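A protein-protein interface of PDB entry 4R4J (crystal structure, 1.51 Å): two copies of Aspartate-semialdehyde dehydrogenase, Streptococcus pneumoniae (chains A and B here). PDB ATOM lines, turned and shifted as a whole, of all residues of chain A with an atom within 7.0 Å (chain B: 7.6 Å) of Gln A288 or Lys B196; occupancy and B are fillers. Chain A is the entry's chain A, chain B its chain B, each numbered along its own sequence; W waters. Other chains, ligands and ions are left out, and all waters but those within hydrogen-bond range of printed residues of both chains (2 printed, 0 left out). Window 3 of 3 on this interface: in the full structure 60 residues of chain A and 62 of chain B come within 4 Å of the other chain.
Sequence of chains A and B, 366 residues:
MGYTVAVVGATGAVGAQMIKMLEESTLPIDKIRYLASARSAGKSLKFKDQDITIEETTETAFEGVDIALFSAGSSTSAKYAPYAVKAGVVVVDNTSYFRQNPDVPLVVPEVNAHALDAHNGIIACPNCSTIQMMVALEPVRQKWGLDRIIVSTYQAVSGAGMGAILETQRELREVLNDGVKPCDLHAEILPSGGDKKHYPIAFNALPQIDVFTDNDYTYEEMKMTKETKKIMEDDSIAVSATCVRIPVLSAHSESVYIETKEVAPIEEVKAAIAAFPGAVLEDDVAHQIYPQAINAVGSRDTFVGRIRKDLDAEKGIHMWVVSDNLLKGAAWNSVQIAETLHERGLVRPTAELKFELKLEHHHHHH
CG1 of Val A285 touches CE1 of Phe B212, 3.6 Å away.
O of His A287 touches OH of Tyr B199, 3.6 Å away.
Lys B197 touches Ile A289 (NZ to CD1, 3.4 Å).
Tyr A290 touches Pro B191.
Tyr B199 touches Tyr A290 (CE2 to OH, 3.4 Å).
CZ of Phe B212 touches CE2 of Tyr A290, 3.97 Å away.
CD2 of Tyr B199 touches NE2 of Gln A292, at 3.4 Å.
Gln A292 touches Leu B206.
Water W1 lies within hydrogen-bond range of the backbone carbonyl oxygen of Lys B197 (2.7 Å), the backbone carbonyl oxygen of Ser B192 (2.7 Å), the side-chain amide nitrogen of Gln A288 (3.3 Å) and a ring nitrogen (ND1) of His B198 (3.4 Å).
Water W2 lies within hydrogen-bond range of the side-chain carboxylate (OD1) of Asp B195 (2.9 Å) and the backbone carbonyl oxygen (O) of Ala A286 (3.3 Å).
No position is printed for both chains.
Of the 17 printed residues of chain B, 8 touch a printed residue of chain A.
Hydrophobic or aromatic side chains of chain B within 4 Å of the printed part of chain A: Pro B191, Tyr B199, Leu B206 and Phe B212.
Along chain B the printed residues that touch a printed residue of chain A span positions 191 to 212.
Of the 8 printed residues of chain A, 6 touch a printed residue of chain B.
Printed residues of chain A that touch a printed residue of chain B: Val A285, His A287, Gln A288, Ile A289, Tyr A290 and Gln A292.
Hydrophobic or aromatic side chains of chain A that line the printed part of chain B: Val A285, Ile A289 and Tyr A290.
Among the printed residues, 15 pairs touch across the chains.
Among the printed residues, no Asp or Glu carboxylate lies within 4 Å of a Lys or Arg side-chain nitrogen of the other chain.
The backbone NH of Ile A289 is in hydrogen-bond range of the backbone carbonyl oxygen of Asp A284, at 2.9 Å.
The backbone carbonyl oxygen of Leu B190 is in hydrogen-bond range of the backbone NH of Tyr B199 (2.9 Å).
NE2 of His B198 lies close to O of Asp B195 (3.4 Å).
The side-chain carboxylate (OD2) of Asp B195 lies within hydrogen-bond range of the side-chain amide nitrogen (NE2) of Gln B208 (2.9 Å).
NZ of Lys B197 is in hydrogen-bond range of OH of Tyr B199 (3.2 Å).
The side-chain amide nitrogen of Gln B208 sits at hydrogen-bond distance from the backbone carbonyl oxygen of Asp B210.
Of the printed residues of chain B, Gln A288 touches Asp B195, Lys B196, Lys B197, Tyr B199 and Gln B208.
Printed residues of chain B within 4 Å of Gln A292: Tyr B199 (3.4 Å) and Leu B206 (3.4 Å).
Ile B189 touches none of the printed residues of chain A.
Of the printed residues of chain A, Pro B191 touches Tyr A290 (3.5 Å).
Printed residues of chain A within 4 Å of Lys B196: Gln A288 (3.5 Å).
Printed residues of chain A within 4 Å of Lys B197: His A287, Gln A288 and Ile A289.
Of the printed residues of chain A, Leu B206 touches Gln A292.
Asp B210 touches none of the printed residues of chain A.
Printed residues of chain A within 4 Å of Phe B212: Val A285 (3.6 Å) and Tyr A290 (3.97 Å).
The nearest printed residue of chain B that does not touch Gln A288 is Pro B191 (4.01 Å).
The nearest residue of chain A that does not touch Lys B196 is Ala A286 (5.1 Å).
The side-chain amino group of Lys B197 lies within hydrogen-bond range of the backbone carbonyl oxygen of His A287 (2.9 Å).
The side-chain amide nitrogen of Gln A288 sits close to the side-chain carboxylate of Asp B195, 3.3 Å away.
OE1 of Gln A288 sits at hydrogen-bond distance from N of Lys B196 (3.5 Å).
The side-chain amide oxygen (OE1) of Gln A288 is in hydrogen-bond range of the backbone NH (N) of Lys B197.
The side-chain hydroxyl of Tyr B199 is in hydrogen-bond range of the backbone carbonyl oxygen of Gln A288, at 2.7 Å.
The side-chain amide oxygen (OE1) of Gln B208 lies within hydrogen-bond range of the side-chain amide nitrogen (NE2) of Gln A288.
OE1 of Gln B208 lies within hydrogen-bond range of OH of Tyr A290.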
ATOM      1  N   ASP A 284       1.629 -19.935 -37.399  1.00  0.00           N
ATOM      2  CA  ASP A 284       2.152 -21.293 -37.358  1.00  0.00           C
ATOM      3  C   ASP A 284       1.315 -22.064 -36.355  1.00  0.00           C
ATOM      4  O   ASP A 284       1.669 -22.201 -35.177  1.00  0.00           O
ATOM      5  CB  ASP A 284       3.641 -21.283 -36.997  1.00  0.00           C
ATOM      6  CG  ASP A 284       4.242 -22.676 -36.918  1.00  0.00           C
ATOM      7  OD1 ASP A 284       3.598 -23.659 -37.347  1.00  0.00           O
ATOM      8  OD2 ASP A 284       5.376 -22.779 -36.408  1.00  0.00           O
ATOM      9  N   VAL A 285       0.174 -22.555 -36.829  1.00  0.00           N
ATOM     10  CA  VAL A 285      -0.807 -23.142 -35.925  1.00  0.00           C
ATOM     11  C   VAL A 285      -0.317 -24.440 -35.296  1.00  0.00           C
ATOM     12  O   VAL A 285      -0.720 -24.777 -34.185  1.00  0.00           O
ATOM     13  CB  VAL A 285      -2.200 -23.327 -36.575  1.00  0.00           C
ATOM     14  CG1 VAL A 285      -2.756 -21.983 -37.039  1.00  0.00           C
ATOM     15  CG2 VAL A 285      -2.175 -24.339 -37.712  1.00  0.00           C
ATOM     16  N   ALA A 286       0.580 -25.150 -35.987  1.00  0.00           N
ATOM     17  CA  ALA A 286       1.205 -26.347 -35.416  1.00  0.00           C
ATOM     18  C   ALA A 286       1.919 -26.059 -34.086  1.00  0.00           C
ATOM     19  O   ALA A 286       2.037 -26.944 -33.254  1.00  0.00           O
ATOM     20  CB  ALA A 286       2.173 -26.972 -36.416  1.00  0.00           C
ATOM     21  N   HIS A 287       2.404 -24.824 -33.902  1.00  0.00           N
ATOM     22  CA  HIS A 287       3.022 -24.408 -32.643  1.00  0.00           C
ATOM     23  C   HIS A 287       2.241 -23.283 -31.967  1.00  0.00           C
ATOM     24  O   HIS A 287       2.795 -22.521 -31.175  1.00  0.00           O
ATOM     25  CB  HIS A 287       4.476 -24.001 -32.883  1.00  0.00           C
ATOM     26  CG  HIS A 287       5.288 -25.085 -33.517  1.00  0.00           C
ATOM     27  ND1 HIS A 287       5.747 -26.179 -32.816  1.00  0.00           N
ATOM     28  CD2 HIS A 287       5.673 -25.276 -34.800  1.00  0.00           C
ATOM     29  CE1 HIS A 287       6.408 -26.980 -33.632  1.00  0.00           C
ATOM     30  NE2 HIS A 287       6.369 -26.459 -34.844  1.00  0.00           N
ATOM     31  N   GLN A 288       0.946 -23.220 -32.265  1.00  0.00           N
ATOM     32  CA  GLN A 288       0.031 -22.242 -31.669  1.00  0.00           C
ATOM     33  C   GLN A 288       0.549 -20.808 -31.749  1.00  0.00           C
ATOM     34  O   GLN A 288       0.468 -20.048 -30.782  1.00  0.00           O
ATOM     35  CB  GLN A 288      -0.271 -22.593 -30.213  1.00  0.00           C
ATOM     36  CG  GLN A 288      -0.853 -23.979 -30.006  1.00  0.00           C
ATOM     37  CD  GLN A 288      -0.878 -24.348 -28.547  1.00  0.00           C
ATOM     38  OE1 GLN A 288      -0.026 -25.098 -28.077  1.00  0.00           O
ATOM     39  NE2 GLN A 288      -1.835 -23.788 -27.807  1.00  0.00           N
ATOM     40  N   ILE A 289       1.080 -20.453 -32.910  1.00  0.00           N
ATOM     41  CA  ILE A 289       1.587 -19.110 -33.164  1.00  0.00           C
ATOM     42  C   ILE A 289       0.541 -18.304 -33.924  1.00  0.00           C
ATOM     43  O   ILE A 289       0.138 -18.654 -35.042  1.00  0.00           O
ATOM     44  CB  ILE A 289       2.904 -19.129 -33.984  1.00  0.00           C
ATOM     45  CG1 ILE A 289       3.989 -19.948 -33.274  1.00  0.00           C
ATOM     46  CG2 ILE A 289       3.378 -17.710 -34.255  1.00  0.00           C
ATOM     47  CD1 ILE A 289       4.333 -19.471 -31.886  1.00  0.00           C
ATOM     48  N   TYR A 290       0.117 -17.214 -33.295  1.00  0.00           N
ATOM     49  CA  TYR A 290      -0.815 -16.255 -33.874  1.00  0.00           C
ATOM     50  C   TYR A 290      -0.597 -14.901 -33.203  1.00  0.00           C
ATOM     51  O   TYR A 290      -0.019 -14.830 -32.118  1.00  0.00           O
ATOM     52  CB  TYR A 290      -2.275 -16.711 -33.698  1.00  0.00           C
ATOM     53  CG  TYR A 290      -2.516 -17.519 -32.459  1.00  0.00           C
ATOM     54  CD1 TYR A 290      -2.475 -16.935 -31.200  1.00  0.00           C
ATOM     55  CD2 TYR A 290      -2.756 -18.892 -32.542  1.00  0.00           C
ATOM     56  CE1 TYR A 290      -2.691 -17.687 -30.057  1.00  0.00           C
ATOM     57  CE2 TYR A 290      -2.963 -19.651 -31.407  1.00  0.00           C
ATOM     58  CZ  TYR A 290      -2.930 -19.035 -30.159  1.00  0.00           C
ATOM     59  OH  TYR A 290      -3.128 -19.751 -29.004  1.00  0.00           O
ATOM     60  N   GLN A 292      -1.059 -11.751 -30.902  1.00  0.00           N
ATOM     61  CA  GLN A 292      -1.683 -11.542 -29.592  1.00  0.00           C
ATOM     62  C   GLN A 292      -1.449 -10.115 -29.160  1.00  0.00           C
ATOM     63  O   GLN A 292      -0.324  -9.625 -29.232  1.00  0.00           O
ATOM     64  CB  GLN A 292      -1.072 -12.447 -28.537  1.00  0.00           C
ATOM     65  CG  GLN A 292      -1.267 -13.932 -28.766  1.00  0.00           C
ATOM     66  CD  GLN A 292      -0.682 -14.745 -27.624  1.00  0.00           C
ATOM     67  OE1 GLN A 292      -0.752 -14.335 -26.454  1.00  0.00           O
ATOM     68  NE2 GLN A 292      -0.091 -15.895 -27.948  1.00  0.00           N
ATOM     69  N   GLU B 188      -0.768 -21.904 -17.392  1.00  0.00           N
ATOM     70  CA  GLU B 188      -0.773 -23.364 -17.411  1.00  0.00           C
ATOM     71  C   GLU B 188      -1.998 -23.973 -18.104  1.00  0.00           C
ATOM     72  O   GLU B 188      -1.985 -25.149 -18.446  1.00  0.00           O
ATOM     73  CB  GLU B 188      -0.716 -23.895 -15.973  1.00  0.00           C
ATOM     74  CG  GLU B 188       0.637 -23.745 -15.296  1.00  0.00           C
ATOM     75  CD  GLU B 188       0.649 -24.302 -13.882  1.00  0.00           C
ATOM     76  OE1 GLU B 188      -0.354 -24.129 -13.155  1.00  0.00           O
ATOM     77  OE2 GLU B 188       1.664 -24.911 -13.494  1.00  0.00           O
ATOM     78  N   ILE B 189      -3.058 -23.191 -18.316  1.00  0.00           N
ATOM     79  CA  ILE B 189      -4.309 -23.751 -18.839  1.00  0.00           C
ATOM     80  C   ILE B 189      -4.687 -23.151 -20.197  1.00  0.00           C
ATOM     81  O   ILE B 189      -4.692 -23.857 -21.197  1.00  0.00           O
ATOM     82  CB  ILE B 189      -5.471 -23.589 -17.830  1.00  0.00           C
ATOM     83  CG1 ILE B 189      -5.137 -24.351 -16.537  1.00  0.00           C
ATOM     84  CG2 ILE B 189      -6.782 -24.076 -18.439  1.00  0.00           C
ATOM     85  CD1 ILE B 189      -6.148 -24.200 -15.426  1.00  0.00           C
ATOM     86  N   LEU B 190      -5.029 -21.866 -20.224  1.00  0.00           N
ATOM     87  CA  LEU B 190      -5.463 -21.225 -21.467  1.00  0.00           C
ATOM     88  C   LEU B 190      -4.307 -21.115 -22.474  1.00  0.00           C
ATOM     89  O   LEU B 190      -3.144 -21.042 -22.091  1.00  0.00           O
ATOM     90  CB  LEU B 190      -6.078 -19.849 -21.191  1.00  0.00           C
ATOM     91  CG  LEU B 190      -7.382 -19.881 -20.387  1.00  0.00           C
ATOM     92  CD1 LEU B 190      -7.725 -18.488 -19.879  1.00  0.00           C
ATOM     93  CD2 LEU B 190      -8.520 -20.488 -21.195  1.00  0.00           C
ATOM     94  N   PRO B 191      -4.622 -21.116 -23.771  1.00  0.00           N
ATOM     95  CA  PRO B 191      -5.963 -21.167 -24.360  1.00  0.00           C
ATOM     96  C   PRO B 191      -6.654 -22.532 -24.296  1.00  0.00           C
ATOM     97  O   PRO B 191      -7.879 -22.574 -24.294  1.00  0.00           O
ATOM     98  CB  PRO B 191      -5.720 -20.765 -25.809  1.00  0.00           C
ATOM     99  CG  PRO B 191      -4.316 -21.157 -26.075  1.00  0.00           C
ATOM    100  CD  PRO B 191      -3.576 -20.954 -24.798  1.00  0.00           C
ATOM    101  N   SER B 192      -5.892 -23.623 -24.245  1.00  0.00           N
ATOM    102  CA  SER B 192      -6.472 -24.969 -24.221  1.00  0.00           C
ATOM    103  C   SER B 192      -5.680 -25.882 -23.288  1.00  0.00           C
ATOM    104  O   SER B 192      -4.481 -26.108 -23.492  1.00  0.00           O
ATOM    105  CB  SER B 192      -6.505 -25.553 -25.633  1.00  0.00           C
ATOM    106  OG  SER B 192      -6.714 -26.956 -25.605  1.00  0.00           O
ATOM    107  N   GLY B 193      -6.352 -26.402 -22.266  1.00  0.00           N
ATOM    108  CA  GLY B 193      -5.705 -27.217 -21.241  1.00  0.00           C
ATOM    109  C   GLY B 193      -4.878 -28.351 -21.802  1.00  0.00           C
ATOM    110  O   GLY B 193      -3.766 -28.595 -21.347  1.00  0.00           O
ATOM    111  N   GLY B 194      -5.424 -29.022 -22.811  1.00  0.00           N
ATOM    112  CA  GLY B 194      -4.805 -30.208 -23.389  1.00  0.00           C
ATOM    113  C   GLY B 194      -3.746 -29.942 -24.444  1.00  0.00           C
ATOM    114  O   GLY B 194      -3.034 -30.865 -24.840  1.00  0.00           O
ATOM    115  N   ASP B 195      -3.632 -28.694 -24.903  1.00  0.00           N
ATOM    116  CA  ASP B 195      -2.638 -28.369 -25.928  1.00  0.00           C
ATOM    117  C   ASP B 195      -1.257 -28.134 -25.292  1.00  0.00           C
ATOM    118  O   ASP B 195      -1.114 -28.103 -24.070  1.00  0.00           O
ATOM    119  CB  ASP B 195      -3.087 -27.159 -26.767  1.00  0.00           C
ATOM    120  CG  ASP B 195      -2.652 -27.249 -28.234  1.00  0.00           C
ATOM    121  OD1 ASP B 195      -1.716 -28.025 -28.554  1.00  0.00           O
ATOM    122  OD2 ASP B 195      -3.245 -26.528 -29.066  1.00  0.00           O
ATOM    123  N   LYS B 196      -0.249 -27.973 -26.141  1.00  0.00           N
ATOM    124  CA  LYS B 196       1.157 -27.990 -25.717  1.00  0.00           C
ATOM    125  C   LYS B 196       1.640 -26.717 -25.032  1.00  0.00           C
ATOM    126  O   LYS B 196       2.421 -26.774 -24.088  1.00  0.00           O
ATOM    127  CB  LYS B 196       2.057 -28.267 -26.925  1.00  0.00           C
ATOM    128  CG  LYS B 196       1.777 -29.599 -27.590  1.00  0.00           C
ATOM    129  CD  LYS B 196       2.620 -29.787 -28.835  1.00  0.00           C
ATOM    130  CE  LYS B 196       2.211 -31.034 -29.593  1.00  0.00           C
ATOM    131  NZ  LYS B 196       3.121 -31.250 -30.746  1.00  0.00           N
ATOM    132  N   LYS B 197       1.179 -25.570 -25.514  1.00  0.00           N
ATOM    133  CA  LYS B 197       1.674 -24.285 -25.053  1.00  0.00           C
ATOM    134  C   LYS B 197       0.549 -23.478 -24.456  1.00  0.00           C
ATOM    135  O   LYS B 197      -0.573 -23.542 -24.937  1.00  0.00           O
ATOM    136  CB  LYS B 197       2.288 -23.528 -26.219  1.00  0.00           C
ATOM    137  CG  LYS B 197       3.528 -24.218 -26.769  1.00  0.00           C
ATOM    138  CD  LYS B 197       3.965 -23.617 -28.086  1.00  0.00           C
ATOM    139  CE  LYS B 197       4.489 -22.209 -27.918  1.00  0.00           C
ATOM    140  NZ  LYS B 197       4.774 -21.641 -29.264  1.00  0.00           N
ATOM    141  N   HIS B 198       0.853 -22.719 -23.412  1.00  0.00           N
ATOM    142  CA  HIS B 198      -0.154 -21.953 -22.708  1.00  0.00           C
ATOM    143  C   HIS B 198       0.248 -20.487 -22.671  1.00  0.00           C
ATOM    144  O   HIS B 198       1.422 -20.172 -22.568  1.00  0.00           O
ATOM    145  CB  HIS B 198      -0.345 -22.538 -21.316  1.00  0.00           C
ATOM    146  CG  HIS B 198      -0.608 -24.005 -21.343  1.00  0.00           C
ATOM    147  ND1 HIS B 198      -1.837 -24.534 -21.672  1.00  0.00           N
ATOM    148  CD2 HIS B 198       0.224 -25.056 -21.172  1.00  0.00           C
ATOM    149  CE1 HIS B 198      -1.759 -25.855 -21.656  1.00  0.00           C
ATOM    150  NE2 HIS B 198      -0.518 -26.195 -21.361  1.00  0.00           N
ATOM    151  N   TYR B 199      -0.742 -19.608 -22.783  1.00  0.00           N
ATOM    152  CA  TYR B 199      -0.516 -18.175 -22.913  1.00  0.00           C
ATOM    153  C   TYR B 199      -1.406 -17.416 -21.942  1.00  0.00           C
ATOM    154  O   TYR B 199      -2.489 -17.887 -21.599  1.00  0.00           O
ATOM    155  CB  TYR B 199      -0.837 -17.673 -24.323  1.00  0.00           C
ATOM    156  CG  TYR B 199      -0.093 -18.345 -25.449  1.00  0.00           C
ATOM    157  CD1 TYR B 199       1.297 -18.388 -25.465  1.00  0.00           C
ATOM    158  CD2 TYR B 199      -0.779 -18.924 -26.510  1.00  0.00           C
ATOM    159  CE1 TYR B 199       1.984 -19.001 -26.498  1.00  0.00           C
ATOM    160  CE2 TYR B 199      -0.100 -19.548 -27.552  1.00  0.00           C
ATOM    161  CZ  TYR B 199       1.288 -19.583 -27.542  1.00  0.00           C
ATOM    162  OH  TYR B 199       1.972 -20.198 -28.582  1.00  0.00           O
ATOM    163  N   LEU B 206      -7.169 -14.094 -27.160  1.00  0.00           N
ATOM    164  CA  LEU B 206      -6.531 -15.292 -27.711  1.00  0.00           C
ATOM    165  C   LEU B 206      -7.410 -15.928 -28.778  1.00  0.00           C
ATOM    166  O   LEU B 206      -8.472 -16.470 -28.455  1.00  0.00           O
ATOM    167  CB  LEU B 206      -6.234 -16.309 -26.600  1.00  0.00           C
ATOM    168  CG  LEU B 206      -5.133 -15.960 -25.588  1.00  0.00           C
ATOM    169  CD1 LEU B 206      -5.145 -16.927 -24.415  1.00  0.00           C
ATOM    170  CD2 LEU B 206      -3.764 -15.966 -26.251  1.00  0.00           C
ATOM    171  N   GLN B 208      -7.704 -18.723 -30.137  1.00  0.00           N
ATOM    172  CA  GLN B 208      -7.687 -20.165 -30.085  1.00  0.00           C
ATOM    173  C   GLN B 208      -8.587 -20.613 -28.958  1.00  0.00           C
ATOM    174  O   GLN B 208      -8.362 -20.253 -27.813  1.00  0.00           O
ATOM    175  CB  GLN B 208      -6.281 -20.717 -29.835  1.00  0.00           C
ATOM    176  CG  GLN B 208      -6.276 -22.251 -29.860  1.00  0.00           C
ATOM    177  CD  GLN B 208      -4.963 -22.928 -29.469  1.00  0.00           C
ATOM    178  OE1 GLN B 208      -3.892 -22.318 -29.426  1.00  0.00           O
ATOM    179  NE2 GLN B 208      -5.055 -24.218 -29.191  1.00  0.00           N
ATOM    180  N   ASP B 210     -10.130 -24.505 -27.918  1.00  0.00           N
ATOM    181  CA  ASP B 210      -9.878 -25.916 -28.226  1.00  0.00           C
ATOM    182  C   ASP B 210      -8.592 -26.042 -29.065  1.00  0.00           C
ATOM    183  O   ASP B 210      -7.824 -25.089 -29.195  1.00  0.00           O
ATOM    184  CB  ASP B 210     -11.097 -26.564 -28.916  1.00  0.00           C
ATOM    185  CG  ASP B 210     -11.280 -28.040 -28.541  1.00  0.00           C
ATOM    186  OD1 ASP B 210     -10.330 -28.831 -28.720  1.00  0.00           O
ATOM    187  OD2 ASP B 210     -12.380 -28.415 -28.074  1.00  0.00           O
ATOM    188  N   VAL B 211      -8.339 -27.227 -29.595  1.00  0.00           N
ATOM    189  CA  VAL B 211      -7.126 -27.481 -30.355  1.00  0.00           C
ATOM    190  C   VAL B 211      -7.370 -27.270 -31.841  1.00  0.00           C
ATOM    191  O   VAL B 211      -8.502 -27.153 -32.278  1.00  0.00           O
ATOM    192  CB  VAL B 211      -6.569 -28.885 -30.070  1.00  0.00           C
ATOM    193  CG1 VAL B 211      -6.291 -29.031 -28.584  1.00  0.00           C
ATOM    194  CG2 VAL B 211      -7.500 -29.974 -30.570  1.00  0.00           C
ATOM    195  N   PHE B 212      -6.292 -27.172 -32.608  1.00  0.00           N
ATOM    196  CA  PHE B 212      -6.404 -26.971 -34.045  1.00  0.00           C
ATOM    197  C   PHE B 212      -6.743 -28.275 -34.739  1.00  0.00           C
ATOM    198  O   PHE B 212      -6.259 -29.340 -34.342  1.00  0.00           O
ATOM    199  CB  PHE B 212      -5.112 -26.379 -34.618  1.00  0.00           C
ATOM    200  CG  PHE B 212      -4.976 -24.906 -34.353  1.00  0.00           C
ATOM    201  CD1 PHE B 212      -5.623 -23.992 -35.174  1.00  0.00           C
ATOM    202  CD2 PHE B 212      -4.275 -24.438 -33.256  1.00  0.00           C
ATOM    203  CE1 PHE B 212      -5.551 -22.637 -34.914  1.00  0.00           C
ATOM    204  CE2 PHE B 212      -4.194 -23.078 -32.995  1.00  0.00           C
ATOM    205  CZ  PHE B 212      -4.834 -22.179 -33.824  1.00  0.00           C
HETATM  206  O   HOH W   1      -3.163 -24.156 -24.761  1.00  0.00           O
HETATM  207  O   HOH W   2      -0.027 -27.947 -30.871  1.00  0.00           O
